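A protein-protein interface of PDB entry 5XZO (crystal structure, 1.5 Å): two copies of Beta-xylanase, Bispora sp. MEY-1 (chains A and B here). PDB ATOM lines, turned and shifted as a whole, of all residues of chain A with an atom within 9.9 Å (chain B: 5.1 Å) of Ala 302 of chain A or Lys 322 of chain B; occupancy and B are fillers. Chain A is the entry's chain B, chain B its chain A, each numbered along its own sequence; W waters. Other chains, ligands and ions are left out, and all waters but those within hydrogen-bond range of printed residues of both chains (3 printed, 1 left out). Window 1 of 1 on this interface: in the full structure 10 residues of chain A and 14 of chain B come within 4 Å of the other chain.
The side-chain amino group (NZ) of Lys 322 of chain B is in hydrogen-bond range of the backbone carbonyl oxygen (O) of Thr 300 of chain A (2.8 Å).
N of Lys 322 of chain B sits at hydrogen-bond distance from O of Pro 298 of chain A.
The side-chain hydroxyl of Thr 300 of chain A lies within hydrogen-bond range of the side-chain hydroxyl of Ser 299 of chain A, at 3.4 Å.
The backbone carbonyl oxygen (O) of Leu 309 of chain B lies within hydrogen-bond range of the backbone NH (N) of Lys 323 of chain B, 2.9 Å away.
OG1 of Thr 300 of chain A lies within hydrogen-bond range of O of Trp 296 of chain A.
OG of Ser 299 of chain A sits at hydrogen-bond distance from O of Trp 296 of chain A (2.9 Å).
Among the printed residues, pairs that only touch across the chains: Ser 299 of chain A with Leu 320 of chain B (3.3 Å), Ala 302 of chain A with Lys 323 of chain B (3.5 Å), Ala 302 of chain A with Asp 327 of chain B (3.5 Å), Ala 302 of chain A with Lys 322 of chain B (3.6 Å), Pro 298 of chain A with Val 321 of chain B (3.7 Å), Ser 299 of chain A with Lys 322 of chain B (3.7 Å), Ser 299 of chain A with Phe 310 of chain B (3.8 Å) and Ala 302 of chain A with Ala 324 of chain B (3.9 Å).
Ala 302 of chain A touches four residues of chain B.
Of the printed residues of chain A, Phe 310 of chain B touches Ser 299 (3.8 Å).
Of the printed residues of chain B, Ser 299 of chain A touches Phe 310 (3.8 Å), Leu 320 (3.3 Å) and Lys 322 (3.7 Å).
Of the printed residues of chain A, Asp 327 of chain B touches Ala 302.
Printed residues of chain A within 4 Å of Lys 323 of chain B: Ala 302 (3.5 Å).
Printed residues of chain A within 4 Å of Leu 320 of chain B: Ser 299 (3.3 Å).
Leu 253 of chain A touches none of the printed residues of chain B.
Trp 296 of chain A touches none of the printed residues of chain B.
The nearest printed residue of chain B that does not touch Ala 302 of chain A is Tyr 326 of chain B (5.5 Å).
Of the 9 printed residues of chain B, 7 touch a printed residue of chain A.
Hydrophobic or aromatic side chains of chain B within 4 Å of the printed part of chain A: Phe 310.
No position is printed for both chains.
Of the 10 pairs that touch across the chains among the printed residues, none has its exchanged pair printed and touching as well.
Water W1 lies within hydrogen-bond range of O of Lys 322 of chain B and N of Gly 303 of chain A.
Water W2 lies within hydrogen-bond range of the backbone carbonyl oxygen of Ala 302 of chain A (2.8 Å), the side-chain amide nitrogen of Gln 304 of chain A (3.3 Å) and the side-chain carboxylate of Asp 327 of chain B (3.5 Å).
Water W3 bridges N of Ala 302 of chain A (2.8 Å) and OD1 of Asp 327 of chain B (2.9 Å).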
ATOM      1  N   ARG A 252      22.819 -25.020   3.504  1.00  0.00           N
ATOM      2  CA  ARG A 252      21.630 -24.964   2.668  1.00  0.00           C
ATOM      3  C   ARG A 252      21.687 -25.994   1.537  1.00  0.00           C
ATOM      4  O   ARG A 252      22.753 -26.475   1.144  1.00  0.00           O
ATOM      5  CB  ARG A 252      21.430 -23.554   2.096  1.00  0.00           C
ATOM      6  CG  ARG A 252      22.503 -23.061   1.142  1.00  0.00           C
ATOM      7  CD  ARG A 252      22.330 -21.539   0.917  1.00  0.00           C
ATOM      8  NE  ARG A 252      23.220 -21.013  -0.125  1.00  0.00           N
ATOM      9  CZ  ARG A 252      24.380 -20.401   0.112  1.00  0.00           C
ATOM     10  NH1 ARG A 252      24.821 -20.238   1.353  1.00  0.00           N
ATOM     11  NH2 ARG A 252      25.126 -19.941  -0.895  1.00  0.00           N
ATOM     12  N   LEU A 253      20.502 -26.337   1.036  1.00  0.00           N
ATOM     13  CA  LEU A 253      20.311 -27.349   0.007  1.00  0.00           C
ATOM     14  C   LEU A 253      19.531 -26.772  -1.163  1.00  0.00           C
ATOM     15  O   LEU A 253      18.769 -25.813  -1.017  1.00  0.00           O
ATOM     16  CB  LEU A 253      19.537 -28.582   0.537  1.00  0.00           C
ATOM     17  CG  LEU A 253      20.123 -29.580   1.530  1.00  0.00           C
ATOM     18  CD1 LEU A 253      20.525 -29.001   2.887  1.00  0.00           C
ATOM     19  CD2 LEU A 253      19.131 -30.710   1.697  1.00  0.00           C
ATOM     20  N   TYR A 254      19.712 -27.383  -2.330  1.00  0.00           N
ATOM     21  CA  TYR A 254      18.818 -27.122  -3.445  1.00  0.00           C
ATOM     22  C   TYR A 254      17.539 -27.914  -3.214  1.00  0.00           C
ATOM     23  O   TYR A 254      17.581 -29.122  -2.970  1.00  0.00           O
ATOM     24  CB  TYR A 254      19.488 -27.483  -4.778  1.00  0.00           C
ATOM     25  CG  TYR A 254      20.804 -26.769  -4.985  1.00  0.00           C
ATOM     26  CD1 TYR A 254      20.844 -25.478  -5.500  1.00  0.00           C
ATOM     27  CD2 TYR A 254      22.008 -27.376  -4.640  1.00  0.00           C
ATOM     28  CE1 TYR A 254      22.051 -24.817  -5.676  1.00  0.00           C
ATOM     29  CE2 TYR A 254      23.212 -26.728  -4.806  1.00  0.00           C
ATOM     30  CZ  TYR A 254      23.231 -25.448  -5.328  1.00  0.00           C
ATOM     31  OH  TYR A 254      24.447 -24.815  -5.490  1.00  0.00           O
ATOM     32  N   LEU A 255      16.415 -27.233  -3.254  1.00  0.00           N
ATOM     33  CA  LEU A 255      15.138 -27.841  -2.936  1.00  0.00           C
ATOM     34  C   LEU A 255      14.599 -28.650  -4.118  1.00  0.00           C
ATOM     35  O   LEU A 255      14.817 -28.286  -5.280  1.00  0.00           O
ATOM     36  CB  LEU A 255      14.134 -26.769  -2.552  1.00  0.00           C
ATOM     37  CG  LEU A 255      14.553 -25.934  -1.345  1.00  0.00           C
ATOM     38  CD1 LEU A 255      13.477 -24.884  -1.065  1.00  0.00           C
ATOM     39  CD2 LEU A 255      14.792 -26.804  -0.123  1.00  0.00           C
ATOM     40  N   PRO A 256      13.895 -29.763  -3.846  1.00  0.00           N
ATOM     41  CA  PRO A 256      13.644 -30.297  -2.500  1.00  0.00           C
ATOM     42  C   PRO A 256      14.791 -31.157  -1.977  1.00  0.00           C
ATOM     43  O   PRO A 256      15.553 -31.694  -2.781  1.00  0.00           O
ATOM     44  CB  PRO A 256      12.388 -31.149  -2.696  1.00  0.00           C
ATOM     45  CG  PRO A 256      12.495 -31.633  -4.093  1.00  0.00           C
ATOM     46  CD  PRO A 256      13.219 -30.562  -4.887  1.00  0.00           C
ATOM     47  N   SER A 295      14.513 -18.854   8.320  1.00  0.00           N
ATOM     48  CA  SER A 295      15.855 -18.756   7.771  1.00  0.00           C
ATOM     49  C   SER A 295      15.924 -17.673   6.702  1.00  0.00           C
ATOM     50  O   SER A 295      14.980 -17.473   5.929  1.00  0.00           O
ATOM     51  CB  SER A 295      16.273 -20.096   7.169  1.00  0.00           C
ATOM     52  OG  SER A 295      17.541 -19.992   6.539  1.00  0.00           O
ATOM     53  N   TRP A 296      17.075 -17.000   6.656  1.00  0.00           N
ATOM     54  CA  TRP A 296      17.356 -16.004   5.626  1.00  0.00           C
ATOM     55  C   TRP A 296      17.432 -16.595   4.221  1.00  0.00           C
ATOM     56  O   TRP A 296      17.311 -15.845   3.242  1.00  0.00           O
ATOM     57  CB  TRP A 296      18.668 -15.302   5.940  1.00  0.00           C
ATOM     58  CG  TRP A 296      19.874 -16.161   5.752  1.00  0.00           C
ATOM     59  CD1 TRP A 296      20.238 -17.264   6.479  1.00  0.00           C
ATOM     60  CD2 TRP A 296      20.906 -15.955   4.797  1.00  0.00           C
ATOM     61  NE1 TRP A 296      21.432 -17.770   6.011  1.00  0.00           N
ATOM     62  CE2 TRP A 296      21.861 -16.979   4.976  1.00  0.00           C
ATOM     63  CE3 TRP A 296      21.118 -14.999   3.797  1.00  0.00           C
ATOM     64  CZ2 TRP A 296      23.004 -17.073   4.198  1.00  0.00           C
ATOM     65  CZ3 TRP A 296      22.254 -15.093   3.025  1.00  0.00           C
ATOM     66  CH2 TRP A 296      23.186 -16.122   3.228  1.00  0.00           C
ATOM     67  N   VAL A 297      17.614 -17.910   4.080  1.00  0.00           N
ATOM     68  CA  VAL A 297      18.024 -18.457   2.783  1.00  0.00           C
ATOM     69  C   VAL A 297      16.979 -18.248   1.689  1.00  0.00           C
ATOM     70  O   VAL A 297      17.346 -17.788   0.601  1.00  0.00           O
ATOM     71  CB  VAL A 297      18.457 -19.923   2.929  1.00  0.00           C
ATOM     72  CG1 VAL A 297      18.525 -20.611   1.558  1.00  0.00           C
ATOM     73  CG2 VAL A 297      19.806 -19.995   3.626  1.00  0.00           C
ATOM     74  N   PRO A 298      15.695 -18.579   1.884  1.00  0.00           N
ATOM     75  CA  PRO A 298      14.761 -18.497   0.741  1.00  0.00           C
ATOM     76  C   PRO A 298      14.545 -17.095   0.198  1.00  0.00           C
ATOM     77  O   PRO A 298      14.211 -16.947  -0.988  1.00  0.00           O
ATOM     78  CB  PRO A 298      13.460 -19.081   1.310  1.00  0.00           C
ATOM     79  CG  PRO A 298      13.928 -19.997   2.411  1.00  0.00           C
ATOM     80  CD  PRO A 298      15.073 -19.265   3.034  1.00  0.00           C
ATOM     81  N   SER A 299      14.709 -16.061   1.016  1.00  0.00           N
ATOM     82  CA  SER A 299      14.568 -14.702   0.503  1.00  0.00           C
ATOM     83  C   SER A 299      15.743 -14.303  -0.371  1.00  0.00           C
ATOM     84  O   SER A 299      15.627 -13.355  -1.152  1.00  0.00           O
ATOM     85  CB  SER A 299      14.436 -13.717   1.662  1.00  0.00           C
ATOM     86  OG  SER A 299      15.641 -13.643   2.401  1.00  0.00           O
ATOM     87  N   THR A 300      16.856 -15.023  -0.278  1.00  0.00           N
ATOM     88  CA  THR A 300      18.119 -14.626  -0.888  1.00  0.00           C
ATOM     89  C   THR A 300      18.512 -15.507  -2.062  1.00  0.00           C
ATOM     90  O   THR A 300      18.984 -15.000  -3.091  1.00  0.00           O
ATOM     91  CB  THR A 300      19.230 -14.650   0.176  1.00  0.00           C
ATOM     92  OG1 THR A 300      18.875 -13.747   1.231  1.00  0.00           O
ATOM     93  CG2 THR A 300      20.570 -14.223  -0.408  1.00  0.00           C
ATOM     94  N   PHE A 301      18.327 -16.817  -1.937  1.00  0.00           N
ATOM     95  CA  PHE A 301      18.744 -17.776  -2.956  1.00  0.00           C
ATOM     96  C   PHE A 301      17.511 -18.514  -3.456  1.00  0.00           C
ATOM     97  O   PHE A 301      16.905 -19.301  -2.717  1.00  0.00           O
ATOM     98  CB  PHE A 301      19.772 -18.776  -2.410  1.00  0.00           C
ATOM     99  CG  PHE A 301      20.936 -18.154  -1.665  1.00  0.00           C
ATOM    100  CD1 PHE A 301      22.044 -17.694  -2.344  1.00  0.00           C
ATOM    101  CD2 PHE A 301      20.930 -18.071  -0.276  1.00  0.00           C
ATOM    102  CE1 PHE A 301      23.115 -17.140  -1.665  1.00  0.00           C
ATOM    103  CE2 PHE A 301      21.998 -17.517   0.408  1.00  0.00           C
ATOM    104  CZ  PHE A 301      23.091 -17.054  -0.293  1.00  0.00           C
ATOM    105  N   ALA A 302      17.157 -18.295  -4.719  1.00  0.00           N
ATOM    106  CA  ALA A 302      16.006 -18.981  -5.291  1.00  0.00           C
ATOM    107  C   ALA A 302      16.222 -20.488  -5.304  1.00  0.00           C
ATOM    108  O   ALA A 302      17.299 -20.980  -5.656  1.00  0.00           O
ATOM    109  CB  ALA A 302      15.739 -18.490  -6.719  1.00  0.00           C
ATOM    110  N   GLY A 303      15.180 -21.225  -4.921  1.00  0.00           N
ATOM    111  CA  GLY A 303      15.253 -22.672  -4.980  1.00  0.00           C
ATOM    112  C   GLY A 303      16.167 -23.314  -3.964  1.00  0.00           C
ATOM    113  O   GLY A 303      16.537 -24.480  -4.136  1.00  0.00           O
ATOM    114  N   GLN A 304      16.571 -22.588  -2.929  1.00  0.00           N
ATOM    115  CA  GLN A 304      17.400 -23.157  -1.875  1.00  0.00           C
ATOM    116  C   GLN A 304      16.729 -22.950  -0.528  1.00  0.00           C
ATOM    117  O   GLN A 304      15.919 -22.040  -0.345  1.00  0.00           O
ATOM    118  CB  GLN A 304      18.794 -22.535  -1.851  1.00  0.00           C
ATOM    119  CG  GLN A 304      19.573 -22.676  -3.170  1.00  0.00           C
ATOM    120  CD  GLN A 304      20.943 -22.047  -3.065  1.00  0.00           C
ATOM    121  OE1 GLN A 304      21.518 -22.007  -1.982  1.00  0.00           O
ATOM    122  NE2 GLN A 304      21.460 -21.528  -4.168  1.00  0.00           N
ATOM    123  N   GLY A 305      17.084 -23.816   0.417  1.00  0.00           N
ATOM    124  CA  GLY A 305      16.522 -23.719   1.753  1.00  0.00           C
ATOM    125  C   GLY A 305      16.913 -24.922   2.587  1.00  0.00           C
ATOM    126  O   GLY A 305      18.006 -25.486   2.422  1.00  0.00           O
ATOM    127  N   LEU B 309       8.358 -11.624  -9.014  1.00  0.00           N
ATOM    128  CA  LEU B 309       9.650 -12.250  -8.738  1.00  0.00           C
ATOM    129  C   LEU B 309       9.750 -12.864  -7.342  1.00  0.00           C
ATOM    130  O   LEU B 309      10.581 -13.760  -7.136  1.00  0.00           O
ATOM    131  CB  LEU B 309      10.775 -11.230  -8.901  1.00  0.00           C
ATOM    132  CG  LEU B 309      10.919 -10.695 -10.322  1.00  0.00           C
ATOM    133  CD1 LEU B 309      12.120  -9.754 -10.356  1.00  0.00           C
ATOM    134  CD2 LEU B 309      11.085 -11.834 -11.335  1.00  0.00           C
ATOM    135  N   PHE B 310       8.964 -12.380  -6.382  1.00  0.00           N
ATOM    136  CA  PHE B 310       8.943 -12.887  -5.015  1.00  0.00           C
ATOM    137  C   PHE B 310       7.508 -13.187  -4.622  1.00  0.00           C
ATOM    138  O   PHE B 310       6.567 -12.637  -5.204  1.00  0.00           O
ATOM    139  CB  PHE B 310       9.477 -11.885  -3.999  1.00  0.00           C
ATOM    140  CG  PHE B 310      10.920 -11.491  -4.193  1.00  0.00           C
ATOM    141  CD1 PHE B 310      11.910 -12.018  -3.372  1.00  0.00           C
ATOM    142  CD2 PHE B 310      11.275 -10.534  -5.129  1.00  0.00           C
ATOM    143  CE1 PHE B 310      13.247 -11.627  -3.511  1.00  0.00           C
ATOM    144  CE2 PHE B 310      12.605 -10.146  -5.271  1.00  0.00           C
ATOM    145  CZ  PHE B 310      13.578 -10.700  -4.468  1.00  0.00           C
ATOM    146  N   LEU B 320       9.849 -12.970   2.568  1.00  0.00           N
ATOM    147  CA  LEU B 320       9.772 -13.157   1.128  1.00  0.00           C
ATOM    148  C   LEU B 320      10.425 -14.469   0.723  1.00  0.00           C
ATOM    149  O   LEU B 320      11.350 -14.959   1.380  1.00  0.00           O
ATOM    150  CB  LEU B 320      10.505 -12.023   0.411  1.00  0.00           C
ATOM    151  CG  LEU B 320       9.842 -10.731  -0.059  1.00  0.00           C
ATOM    152  CD1 LEU B 320       8.834 -10.250   0.920  1.00  0.00           C
ATOM    153  CD2 LEU B 320      10.927  -9.682  -0.253  1.00  0.00           C
ATOM    154  N   VAL B 321       9.970 -15.013  -0.397  1.00  0.00           N
ATOM    155  CA  VAL B 321      10.644 -16.132  -1.046  1.00  0.00           C
ATOM    156  C   VAL B 321      10.979 -15.698  -2.462  1.00  0.00           C
ATOM    157  O   VAL B 321      10.091 -15.281  -3.219  1.00  0.00           O
ATOM    158  CB  VAL B 321       9.797 -17.411  -1.032  1.00  0.00           C
ATOM    159  CG1 VAL B 321      10.481 -18.518  -1.839  1.00  0.00           C
ATOM    160  CG2 VAL B 321       9.581 -17.851   0.402  1.00  0.00           C
ATOM    161  N   LYS B 322      12.265 -15.761  -2.798  1.00  0.00           N
ATOM    162  CA  LYS B 322      12.731 -15.392  -4.125  1.00  0.00           C
ATOM    163  C   LYS B 322      12.420 -16.519  -5.096  1.00  0.00           C
ATOM    164  O   LYS B 322      12.713 -17.683  -4.812  1.00  0.00           O
ATOM    165  CB  LYS B 322      14.234 -15.107  -4.073  1.00  0.00           C
ATOM    166  CG  LYS B 322      14.865 -14.787  -5.427  1.00  0.00           C
ATOM    167  CD  LYS B 322      16.374 -14.579  -5.298  1.00  0.00           C
ATOM    168  CE  LYS B 322      16.721 -13.153  -4.798  1.00  0.00           C
ATOM    169  NZ  LYS B 322      18.203 -12.876  -4.713  1.00  0.00           N
ATOM    170  N   LYS B 323      11.817 -16.188  -6.233  1.00  0.00           N
ATOM    171  CA  LYS B 323      11.459 -17.201  -7.218  1.00  0.00           C
ATOM    172  C   LYS B 323      12.580 -17.414  -8.229  1.00  0.00           C
ATOM    173  O   LYS B 323      13.425 -16.542  -8.444  1.00  0.00           O
ATOM    174  CB  LYS B 323      10.196 -16.806  -7.977  1.00  0.00           C
ATOM    175  CG  LYS B 323       8.936 -16.729  -7.166  1.00  0.00           C
ATOM    176  CD  LYS B 323       7.779 -16.527  -8.138  1.00  0.00           C
ATOM    177  CE  LYS B 323       6.559 -16.013  -7.426  1.00  0.00           C
ATOM    178  NZ  LYS B 323       5.496 -15.640  -8.432  1.00  0.00           N
ATOM    179  N   ALA B 324      12.547 -18.580  -8.891  1.00  0.00           N
ATOM    180  CA  ALA B 324      13.484 -18.831  -9.980  1.00  0.00           C
ATOM    181  C   ALA B 324      13.423 -17.739 -11.046  1.00  0.00           C
ATOM    182  O   ALA B 324      14.439 -17.445 -11.687  1.00  0.00           O
ATOM    183  CB  ALA B 324      13.215 -20.200 -10.606  1.00  0.00           C
ATOM    184  N   TYR B 326      13.462 -14.640 -10.686  1.00  0.00           N
ATOM    185  CA  TYR B 326      14.472 -13.641 -10.364  1.00  0.00           C
ATOM    186  C   TYR B 326      15.788 -13.960 -11.063  1.00  0.00           C
ATOM    187  O   TYR B 326      16.431 -13.076 -11.641  1.00  0.00           O
ATOM    188  CB  TYR B 326      14.676 -13.581  -8.842  1.00  0.00           C
ATOM    189  CG  TYR B 326      15.778 -12.640  -8.391  1.00  0.00           C
ATOM    190  CD1 TYR B 326      15.481 -11.376  -7.905  1.00  0.00           C
ATOM    191  CD2 TYR B 326      17.121 -13.020  -8.444  1.00  0.00           C
ATOM    192  CE1 TYR B 326      16.476 -10.506  -7.501  1.00  0.00           C
ATOM    193  CE2 TYR B 326      18.124 -12.158  -8.047  1.00  0.00           C
ATOM    194  CZ  TYR B 326      17.804 -10.905  -7.576  1.00  0.00           C
ATOM    195  OH  TYR B 326      18.801 -10.048  -7.168  1.00  0.00           O
ATOM    196  N   ASP B 327      16.215 -15.223 -10.985  1.00  0.00           N
ATOM    197  CA  ASP B 327      17.476 -15.622 -11.600  1.00  0.00           C
ATOM    198  C   ASP B 327      17.402 -15.546 -13.117  1.00  0.00           C
ATOM    199  O   ASP B 327      18.425 -15.299 -13.762  1.00  0.00           O
ATOM    200  CB  ASP B 327      17.860 -17.029 -11.151  1.00  0.00           C
ATOM    201  CG  ASP B 327      18.299 -17.083  -9.688  1.00  0.00           C
ATOM    202  OD1 ASP B 327      18.668 -16.033  -9.125  1.00  0.00           O
ATOM    203  OD2 ASP B 327      18.310 -18.201  -9.136  1.00  0.00           O
HETATM  204  O   HOH W   1      12.507 -20.367  -5.186  1.00  0.00           O
HETATM  205  O   HOH W   2      19.812 -20.211  -6.697  1.00  0.00           O
HETATM  206  O   HOH W   3      18.982 -16.915  -6.414  1.00  0.00           O
